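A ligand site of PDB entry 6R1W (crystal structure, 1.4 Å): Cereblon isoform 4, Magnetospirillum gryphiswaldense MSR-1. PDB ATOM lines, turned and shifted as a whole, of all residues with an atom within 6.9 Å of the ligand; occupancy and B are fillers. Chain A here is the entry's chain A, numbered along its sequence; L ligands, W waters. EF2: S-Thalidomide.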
ATOM      1  N   VAL A  49      29.951 -24.838 -31.831  1.00  0.00           N
ATOM      2  CA  VAL A  49      30.775 -23.680 -31.522  1.00  0.00           C
ATOM      3  C   VAL A  49      31.356 -23.770 -30.148  1.00  0.00           C
ATOM      4  O   VAL A  49      30.888 -24.569 -29.345  1.00  0.00           O
ATOM      5  CB  VAL A  49      29.878 -22.417 -31.587  1.00  0.00           C
ATOM      6  CG1 VAL A  49      29.382 -22.257 -33.036  1.00  0.00           C
ATOM      7  CG2 VAL A  49      28.710 -22.476 -30.586  1.00  0.00           C
ATOM      8  N   PHE A  50      32.390 -22.984 -29.835  1.00  0.00           N
ATOM      9  CA  PHE A  50      32.890 -22.864 -28.475  1.00  0.00           C
ATOM     10  C   PHE A  50      33.060 -21.457 -28.025  1.00  0.00           C
ATOM     11  O   PHE A  50      33.355 -20.568 -28.830  1.00  0.00           O
ATOM     12  CB  PHE A  50      34.170 -23.687 -28.167  1.00  0.00           C
ATOM     13  CG  PHE A  50      35.276 -23.327 -28.923  1.00  0.00           C
ATOM     14  CD1 PHE A  50      35.562 -23.903 -30.217  1.00  0.00           C
ATOM     15  CD2 PHE A  50      36.261 -22.459 -28.388  1.00  0.00           C
ATOM     16  CE1 PHE A  50      36.657 -23.469 -30.952  1.00  0.00           C
ATOM     17  CE2 PHE A  50      37.321 -22.031 -29.109  1.00  0.00           C
ATOM     18  CZ  PHE A  50      37.571 -22.566 -30.385  1.00  0.00           C
ATOM     19  N   ASN A  51      32.867 -21.182 -26.751  1.00  0.00           N
ATOM     20  CA  ASN A  51      33.116 -19.861 -26.191  1.00  0.00           C
ATOM     21  C   ASN A  51      34.552 -19.689 -25.676  1.00  0.00           C
ATOM     22  O   ASN A  51      35.363 -20.609 -25.708  1.00  0.00           O
ATOM     23  CB  ASN A  51      32.019 -19.563 -25.142  1.00  0.00           C
ATOM     24  CG  ASN A  51      32.151 -20.371 -23.875  1.00  0.00           C
ATOM     25  OD1 ASN A  51      33.153 -21.021 -23.611  1.00  0.00           O
ATOM     26  ND2 ASN A  51      31.173 -20.226 -23.043  1.00  0.00           N
ATOM     27  N   PRO A  52      34.862 -18.493 -25.144  1.00  0.00           N
ATOM     28  CA  PRO A  52      36.226 -18.238 -24.655  1.00  0.00           C
ATOM     29  C   PRO A  52      36.599 -19.062 -23.458  1.00  0.00           C
ATOM     30  O   PRO A  52      37.815 -19.241 -23.211  1.00  0.00           O
ATOM     31  CB  PRO A  52      36.222 -16.730 -24.294  1.00  0.00           C
ATOM     32  CG  PRO A  52      35.162 -16.174 -25.227  1.00  0.00           C
ATOM     33  CD  PRO A  52      34.074 -17.201 -25.228  1.00  0.00           C
ATOM     34  N   ALA A  53      35.619 -19.654 -22.782  1.00  0.00           N
ATOM     35  CA  ALA A  53      35.906 -20.579 -21.660  1.00  0.00           C
ATOM     36  C   ALA A  53      35.996 -21.999 -22.147  1.00  0.00           C
ATOM     37  O   ALA A  53      36.113 -22.900 -21.320  1.00  0.00           O
ATOM     38  CB  ALA A  53      34.862 -20.449 -20.601  1.00  0.00           C
ATOM     39  N   MET A  55      33.828 -23.920 -23.613  1.00  0.00           N
ATOM     40  CA  MET A  55      32.604 -24.716 -23.592  1.00  0.00           C
ATOM     41  C   MET A  55      32.109 -24.912 -25.015  1.00  0.00           C
ATOM     42  O   MET A  55      31.985 -23.912 -25.743  1.00  0.00           O
ATOM     43  CB  MET A  55      31.593 -24.038 -22.728  1.00  0.00           C
ATOM     44  CG  MET A  55      30.307 -24.797 -22.474  1.00  0.00           C
ATOM     45  SD  MET A  55      30.387 -26.535 -22.116  1.00  0.00           S
ATOM     46  CE  MET A  55      31.126 -26.558 -20.477  1.00  0.00           C
ATOM     47  N   PHE A  57      29.104 -25.898 -27.623  1.00  0.00           N
ATOM     48  CA  PHE A  57      27.618 -25.848 -27.662  1.00  0.00           C
ATOM     49  C   PHE A  57      27.174 -26.333 -29.041  1.00  0.00           C
ATOM     50  O   PHE A  57      27.723 -25.979 -30.059  1.00  0.00           O
ATOM     51  CB  PHE A  57      27.084 -24.451 -27.449  1.00  0.00           C
ATOM     52  CG  PHE A  57      27.486 -23.757 -26.170  1.00  0.00           C
ATOM     53  CD1 PHE A  57      26.791 -23.981 -25.037  1.00  0.00           C
ATOM     54  CD2 PHE A  57      28.573 -22.905 -26.112  1.00  0.00           C
ATOM     55  CE1 PHE A  57      27.160 -23.351 -23.807  1.00  0.00           C
ATOM     56  CE2 PHE A  57      28.908 -22.292 -24.926  1.00  0.00           C
ATOM     57  CZ  PHE A  57      28.195 -22.454 -23.792  1.00  0.00           C
ATOM     58  N   SER A  75      26.220  -7.410 -27.710  1.00  0.00           N
ATOM     59  CA  SER A  75      27.636  -7.368 -27.913  1.00  0.00           C
ATOM     60  C   SER A  75      28.035  -8.078 -29.166  1.00  0.00           C
ATOM     61  O   SER A  75      27.493  -9.168 -29.425  1.00  0.00           O
ATOM     62  CB  SER A  75      28.332  -8.019 -26.735  1.00  0.00           C
ATOM     63  OG  SER A  75      29.724  -8.027 -26.954  1.00  0.00           O
ATOM     64  N   GLY A  76      28.960  -7.565 -29.931  1.00  0.00           N
ATOM     65  CA  GLY A  76      29.529  -8.290 -31.040  1.00  0.00           C
ATOM     66  C   GLY A  76      30.708  -9.169 -30.662  1.00  0.00           C
ATOM     67  O   GLY A  76      31.204  -9.903 -31.550  1.00  0.00           O
ATOM     68  N   GLU A  77      31.177  -9.130 -29.431  1.00  0.00           N
ATOM     69  CA  GLU A  77      32.422  -9.806 -29.072  1.00  0.00           C
ATOM     70  C   GLU A  77      32.302 -11.304 -29.225  1.00  0.00           C
ATOM     71  O   GLU A  77      31.388 -11.898 -28.725  1.00  0.00           O
ATOM     72  CB  GLU A  77      32.840  -9.460 -27.647  1.00  0.00           C
ATOM     73  CG  GLU A  77      33.176  -8.039 -27.363  1.00  0.00           C
ATOM     74  CD  GLU A  77      33.757  -8.000 -25.921  1.00  0.00           C
ATOM     75  OE1 GLU A  77      33.207  -7.274 -25.067  1.00  0.00           O
ATOM     76  OE2 GLU A  77      34.730  -8.759 -25.634  1.00  0.00           O
ATOM     77  N   PHE A  78      33.221 -11.902 -29.954  1.00  0.00           N
ATOM     78  CA  PHE A  78      33.318 -13.342 -30.082  1.00  0.00           C
ATOM     79  C   PHE A  78      32.080 -13.876 -30.813  1.00  0.00           C
ATOM     80  O   PHE A  78      31.808 -15.069 -30.728  1.00  0.00           O
ATOM     81  CB  PHE A  78      33.507 -14.077 -28.734  1.00  0.00           C
ATOM     82  CG  PHE A  78      34.623 -13.549 -27.874  1.00  0.00           C
ATOM     83  CD1 PHE A  78      35.847 -13.642 -28.219  1.00  0.00           C
ATOM     84  CD2 PHE A  78      34.293 -12.998 -26.636  1.00  0.00           C
ATOM     85  CE1 PHE A  78      36.896 -13.184 -27.396  1.00  0.00           C
ATOM     86  CE2 PHE A  78      35.279 -12.484 -25.789  1.00  0.00           C
ATOM     87  CZ  PHE A  78      36.558 -12.598 -26.172  1.00  0.00           C
ATOM     88  N   SER A  79      31.291 -13.091 -31.528  1.00  0.00           N
ATOM     89  CA  SER A  79      30.085 -13.643 -32.113  1.00  0.00           C
ATOM     90  C   SER A  79      30.378 -14.753 -33.097  1.00  0.00           C
ATOM     91  O   SER A  79      31.260 -14.645 -33.942  1.00  0.00           O
ATOM     92  CB  SER A  79      29.330 -12.542 -32.886  1.00  0.00           C
ATOM     93  OG  SER A  79      28.144 -13.114 -33.395  1.00  0.00           O
ATOM     94  N   TRP A  80      29.603 -15.848 -32.928  1.00  0.00           N
ATOM     95  CA  TRP A  80      29.739 -16.994 -33.819  1.00  0.00           C
ATOM     96  C   TRP A  80      29.108 -16.778 -35.174  1.00  0.00           C
ATOM     97  O   TRP A  80      29.293 -17.619 -36.084  1.00  0.00           O
ATOM     98  CB  TRP A  80      29.135 -18.217 -33.151  1.00  0.00           C
ATOM     99  CG  TRP A  80      29.799 -18.622 -31.911  1.00  0.00           C
ATOM    100  CD1 TRP A  80      31.131 -18.842 -31.710  1.00  0.00           C
ATOM    101  CD2 TRP A  80      29.150 -18.961 -30.689  1.00  0.00           C
ATOM    102  NE1 TRP A  80      31.358 -19.261 -30.393  1.00  0.00           N
ATOM    103  CE2 TRP A  80      30.145 -19.334 -29.758  1.00  0.00           C
ATOM    104  CE3 TRP A  80      27.814 -18.920 -30.244  1.00  0.00           C
ATOM    105  CZ2 TRP A  80      29.807 -19.683 -28.446  1.00  0.00           C
ATOM    106  CZ3 TRP A  80      27.503 -19.312 -29.007  1.00  0.00           C
ATOM    107  CH2 TRP A  80      28.483 -19.711 -28.130  1.00  0.00           C
ATOM    108  N   PHE A  81      28.392 -15.680 -35.352  1.00  0.00           N
ATOM    109  CA  PHE A  81      27.622 -15.449 -36.561  1.00  0.00           C
ATOM    110  C   PHE A  81      28.002 -14.073 -37.102  1.00  0.00           C
ATOM    111  O   PHE A  81      27.715 -13.039 -36.454  1.00  0.00           O
ATOM    112  CB  PHE A  81      26.092 -15.556 -36.315  1.00  0.00           C
ATOM    113  CG  PHE A  81      25.687 -16.936 -35.849  1.00  0.00           C
ATOM    114  CD1 PHE A  81      25.451 -17.953 -36.759  1.00  0.00           C
ATOM    115  CD2 PHE A  81      25.573 -17.227 -34.549  1.00  0.00           C
ATOM    116  CE1 PHE A  81      24.965 -19.224 -36.369  1.00  0.00           C
ATOM    117  CE2 PHE A  81      25.188 -18.494 -34.126  1.00  0.00           C
ATOM    118  CZ  PHE A  81      24.892 -19.485 -35.070  1.00  0.00           C
ATOM    119  N   TYR A  84      26.365 -10.310 -36.617  1.00  0.00           N
ATOM    120  CA  TYR A  84      25.361 -10.278 -35.561  1.00  0.00           C
ATOM    121  C   TYR A  84      25.948 -10.017 -34.206  1.00  0.00           C
ATOM    122  O   TYR A  84      27.039 -10.478 -33.913  1.00  0.00           O
ATOM    123  CB  TYR A  84      24.604 -11.599 -35.488  1.00  0.00           C
ATOM    124  CG  TYR A  84      23.823 -11.965 -36.706  1.00  0.00           C
ATOM    125  CD1 TYR A  84      22.501 -11.569 -36.842  1.00  0.00           C
ATOM    126  CD2 TYR A  84      24.378 -12.685 -37.719  1.00  0.00           C
ATOM    127  CE1 TYR A  84      21.789 -11.883 -37.958  1.00  0.00           C
ATOM    128  CE2 TYR A  84      23.654 -13.020 -38.854  1.00  0.00           C
ATOM    129  CZ  TYR A  84      22.373 -12.634 -38.975  1.00  0.00           C
ATOM    130  OH  TYR A  84      21.685 -12.962 -40.109  1.00  0.00           O
ATOM    131  N   TRP A  86      25.008 -10.280 -30.022  1.00  0.00           N
ATOM    132  CA  TRP A  86      24.222 -11.267 -29.187  1.00  0.00           C
ATOM    133  C   TRP A  86      23.849 -10.640 -27.865  1.00  0.00           C
ATOM    134  O   TRP A  86      24.559  -9.815 -27.289  1.00  0.00           O
ATOM    135  CB  TRP A  86      25.014 -12.511 -28.990  1.00  0.00           C
ATOM    136  CG  TRP A  86      26.385 -12.372 -28.470  1.00  0.00           C
ATOM    137  CD1 TRP A  86      27.571 -12.286 -29.180  1.00  0.00           C
ATOM    138  CD2 TRP A  86      26.793 -12.214 -27.102  1.00  0.00           C
ATOM    139  NE1 TRP A  86      28.603 -12.099 -28.359  1.00  0.00           N
ATOM    140  CE2 TRP A  86      28.194 -11.991 -27.072  1.00  0.00           C
ATOM    141  CE3 TRP A  86      26.115 -12.248 -25.871  1.00  0.00           C
ATOM    142  CZ2 TRP A  86      28.864 -11.794 -25.894  1.00  0.00           C
ATOM    143  CZ3 TRP A  86      26.825 -12.079 -24.707  1.00  0.00           C
ATOM    144  CH2 TRP A  86      28.204 -11.884 -24.708  1.00  0.00           C
ATOM    145  N   THR A  87      22.776 -11.206 -27.316  1.00  0.00           N
ATOM    146  CA  THR A  87      22.277 -10.978 -25.960  1.00  0.00           C
ATOM    147  C   THR A  87      22.069 -12.403 -25.368  1.00  0.00           C
ATOM    148  O   THR A  87      21.522 -13.274 -26.057  1.00  0.00           O
ATOM    149  CB  THR A  87      20.957 -10.195 -26.036  1.00  0.00           C
ATOM    150  OG1 THR A  87      21.356  -8.904 -26.614  1.00  0.00           O
ATOM    151  CG2 THR A  87      20.387  -9.856 -24.843  1.00  0.00           C
ATOM    152  N   ILE A  88      22.431 -12.603 -24.139  1.00  0.00           N
ATOM    153  CA  ILE A  88      22.066 -13.871 -23.418  1.00  0.00           C
ATOM    154  C   ILE A  88      20.598 -14.022 -23.360  1.00  0.00           C
ATOM    155  O   ILE A  88      19.876 -13.062 -22.986  1.00  0.00           O
ATOM    156  CB  ILE A  88      22.753 -13.839 -22.051  1.00  0.00           C
ATOM    157  CG1 ILE A  88      24.273 -14.014 -22.237  1.00  0.00           C
ATOM    158  CG2 ILE A  88      22.197 -14.920 -21.160  1.00  0.00           C
ATOM    159  CD1 ILE A  88      25.064 -13.663 -20.978  1.00  0.00           C
ATOM    160  N   HIS A  97      20.117 -20.941 -18.669  1.00  0.00           N
ATOM    161  CA  HIS A  97      20.679 -20.288 -19.849  1.00  0.00           C
ATOM    162  C   HIS A  97      20.414 -21.136 -21.061  1.00  0.00           C
ATOM    163  O   HIS A  97      21.008 -22.214 -21.244  1.00  0.00           O
ATOM    164  CB  HIS A  97      22.158 -20.070 -19.674  1.00  0.00           C
ATOM    165  CG  HIS A  97      22.781 -19.513 -20.876  1.00  0.00           C
ATOM    166  ND1 HIS A  97      24.117 -19.717 -21.129  1.00  0.00           N
ATOM    167  CD2 HIS A  97      22.282 -18.719 -21.864  1.00  0.00           C
ATOM    168  CE1 HIS A  97      24.379 -19.081 -22.272  1.00  0.00           C
ATOM    169  NE2 HIS A  97      23.313 -18.436 -22.733  1.00  0.00           N
ATOM    170  N   TRP A 100      21.075 -17.613 -26.967  1.00  0.00           N
ATOM    171  CA  TRP A 100      21.386 -16.199 -27.253  1.00  0.00           C
ATOM    172  C   TRP A 100      20.390 -15.734 -28.302  1.00  0.00           C
ATOM    173  O   TRP A 100      19.958 -16.494 -29.144  1.00  0.00           O
ATOM    174  CB  TRP A 100      22.792 -16.003 -27.804  1.00  0.00           C
ATOM    175  CG  TRP A 100      23.873 -16.526 -26.897  1.00  0.00           C
ATOM    176  CD1 TRP A 100      24.520 -15.813 -25.919  1.00  0.00           C
ATOM    177  CD2 TRP A 100      24.330 -17.903 -26.767  1.00  0.00           C
ATOM    178  NE1 TRP A 100      25.374 -16.670 -25.228  1.00  0.00           N
ATOM    179  CE2 TRP A 100      25.267 -17.934 -25.722  1.00  0.00           C
ATOM    180  CE3 TRP A 100      24.057 -19.094 -27.443  1.00  0.00           C
ATOM    181  CZ2 TRP A 100      25.930 -19.144 -25.374  1.00  0.00           C
ATOM    182  CZ3 TRP A 100      24.673 -20.270 -27.023  1.00  0.00           C
ATOM    183  CH2 TRP A 100      25.556 -20.245 -26.042  1.00  0.00           C
ATOM    184  N   TYR A 102      20.291 -13.073 -31.393  1.00  0.00           N
ATOM    185  CA  TYR A 102      21.200 -12.347 -32.327  1.00  0.00           C
ATOM    186  C   TYR A 102      20.428 -11.296 -33.075  1.00  0.00           C
ATOM    187  O   TYR A 102      19.306 -11.501 -33.456  1.00  0.00           O
ATOM    188  CB  TYR A 102      21.794 -13.336 -33.332  1.00  0.00           C
ATOM    189  CG  TYR A 102      22.790 -14.300 -32.669  1.00  0.00           C
ATOM    190  CD1 TYR A 102      24.102 -13.898 -32.492  1.00  0.00           C
ATOM    191  CD2 TYR A 102      22.388 -15.516 -32.158  1.00  0.00           C
ATOM    192  CE1 TYR A 102      25.012 -14.712 -31.869  1.00  0.00           C
ATOM    193  CE2 TYR A 102      23.289 -16.325 -31.491  1.00  0.00           C
ATOM    194  CZ  TYR A 102      24.572 -15.887 -31.353  1.00  0.00           C
ATOM    195  OH  TYR A 102      25.530 -16.746 -30.716  1.00  0.00           O
HETATM  196  O01 EF2 L   1      31.533 -16.841 -27.558  1.00  0.00           O
HETATM  197  C02 EF2 L   1      30.329 -16.444 -27.664  1.00  0.00           C
HETATM  198  N03 EF2 L   1      29.815 -16.208 -28.911  1.00  0.00           N
HETATM  199  C04 EF2 L   1      28.500 -15.881 -29.139  1.00  0.00           C
HETATM  200  O05 EF2 L   1      28.149 -15.796 -30.309  1.00  0.00           O
HETATM  201  C06 EF2 L   1      27.675 -15.745 -27.953  1.00  0.00           C
HETATM  202  C07 EF2 L   1      28.280 -15.628 -26.711  1.00  0.00           C
HETATM  203  C08 EF2 L   1      29.512 -16.259 -26.416  1.00  0.00           C
HETATM  204  N09 EF2 L   1      30.207 -16.198 -25.210  1.00  0.00           N
HETATM  205  C11 EF2 L   1      32.622 -15.168 -21.539  1.00  0.00           C
HETATM  206  C12 EF2 L   1      32.332 -14.659 -22.805  1.00  0.00           C
HETATM  207  C13 EF2 L   1      31.476 -15.386 -23.624  1.00  0.00           C
HETATM  208  C14 EF2 L   1      30.922 -16.573 -23.167  1.00  0.00           C
HETATM  209  O16 EF2 L   1      31.472 -14.190 -25.938  1.00  0.00           O
HETATM  210  O18 EF2 L   1      29.336 -18.190 -24.069  1.00  0.00           O
HETATM  211  C19 EF2 L   1      31.215 -17.082 -21.888  1.00  0.00           C
HETATM  212  C20 EF2 L   1      32.110 -16.384 -21.081  1.00  0.00           C
HETATM  213  C3  EF2 L   1      30.016 -17.011 -24.160  1.00  0.00           C
HETATM  214  C4  EF2 L   1      30.932 -14.986 -24.922  1.00  0.00           C
HETATM  215  O   HOH W   1      27.728 -18.954 -22.173  1.00  0.00           O
HETATM  216  O   HOH W   2      27.126 -16.090 -23.080  1.00  0.00           O
HETATM  217  O   HOH W   3      31.846 -11.481 -24.137  1.00  0.00           O
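The backbone NH of Ala 53 is in hydrogen-bond range of the side-chain amide oxygen of Asn 51 (2.9 Å). N of Met 55 is in hydrogen-bond range of OD1 of Asn 51, at 3.0 Å. The indole nitrogen of Trp 80 is in hydrogen-bond range of the backbone carbonyl oxygen of Phe 50. O of Phe 81 is in hydrogen-bond range of OG of Ser 79 (3.1 Å). The side-chain hydroxyl (OG) of Ser 79 lies within hydrogen-bond range of the backbone carbonyl oxygen (O) of Tyr 84 (2.9 Å). O of Glu 77 lies within hydrogen-bond range of NE1 of Trp 86, 2.8 Å away. The backbone carbonyl oxygen (O) of Ser 75 is in hydrogen-bond range of the backbone NH (N) of Trp 86 (2.8 Å). The side-chain hydroxyl (OG) of Ser 75 lies within hydrogen-bond range of the backbone NH (N) of Glu 77 (3.1 Å).
CD of Pro 52 touches O01 of the ligand, at 3.5 Å. O of Glu 77 touches O16 of the ligand (3.6 Å). CA of Ser 79 touches O05 of the ligand (3.4 Å). Trp 86 touches the ligand. Trp 100 touches the ligand (NE1 to C07, 3.4 Å). Hydrophobic or aromatic side chains within 4 Å of the ligand: Pro 52, Phe 78, Trp 80, Trp 86, Trp 100 and Tyr 102. The nearest printed residue that does not touch the ligand is Phe 57 (4.2 Å).
O05 of the ligand is in hydrogen-bond range of OH of Tyr 102 (2.8 Å). An oxygen (O18) of the ligand lies within hydrogen-bond range of the side-chain amide nitrogen of Asn 51 (2.9 Å). The backbone carbonyl oxygen of Phe 78 sits at hydrogen-bond distance from a nitrogen (N03) of the ligand (2.9 Å). N of Trp 80 lies within hydrogen-bond range of O05 of the ligand.
Water W2 bridges the indole nitrogen of Trp 100 and an oxygen (O18) of the ligand.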
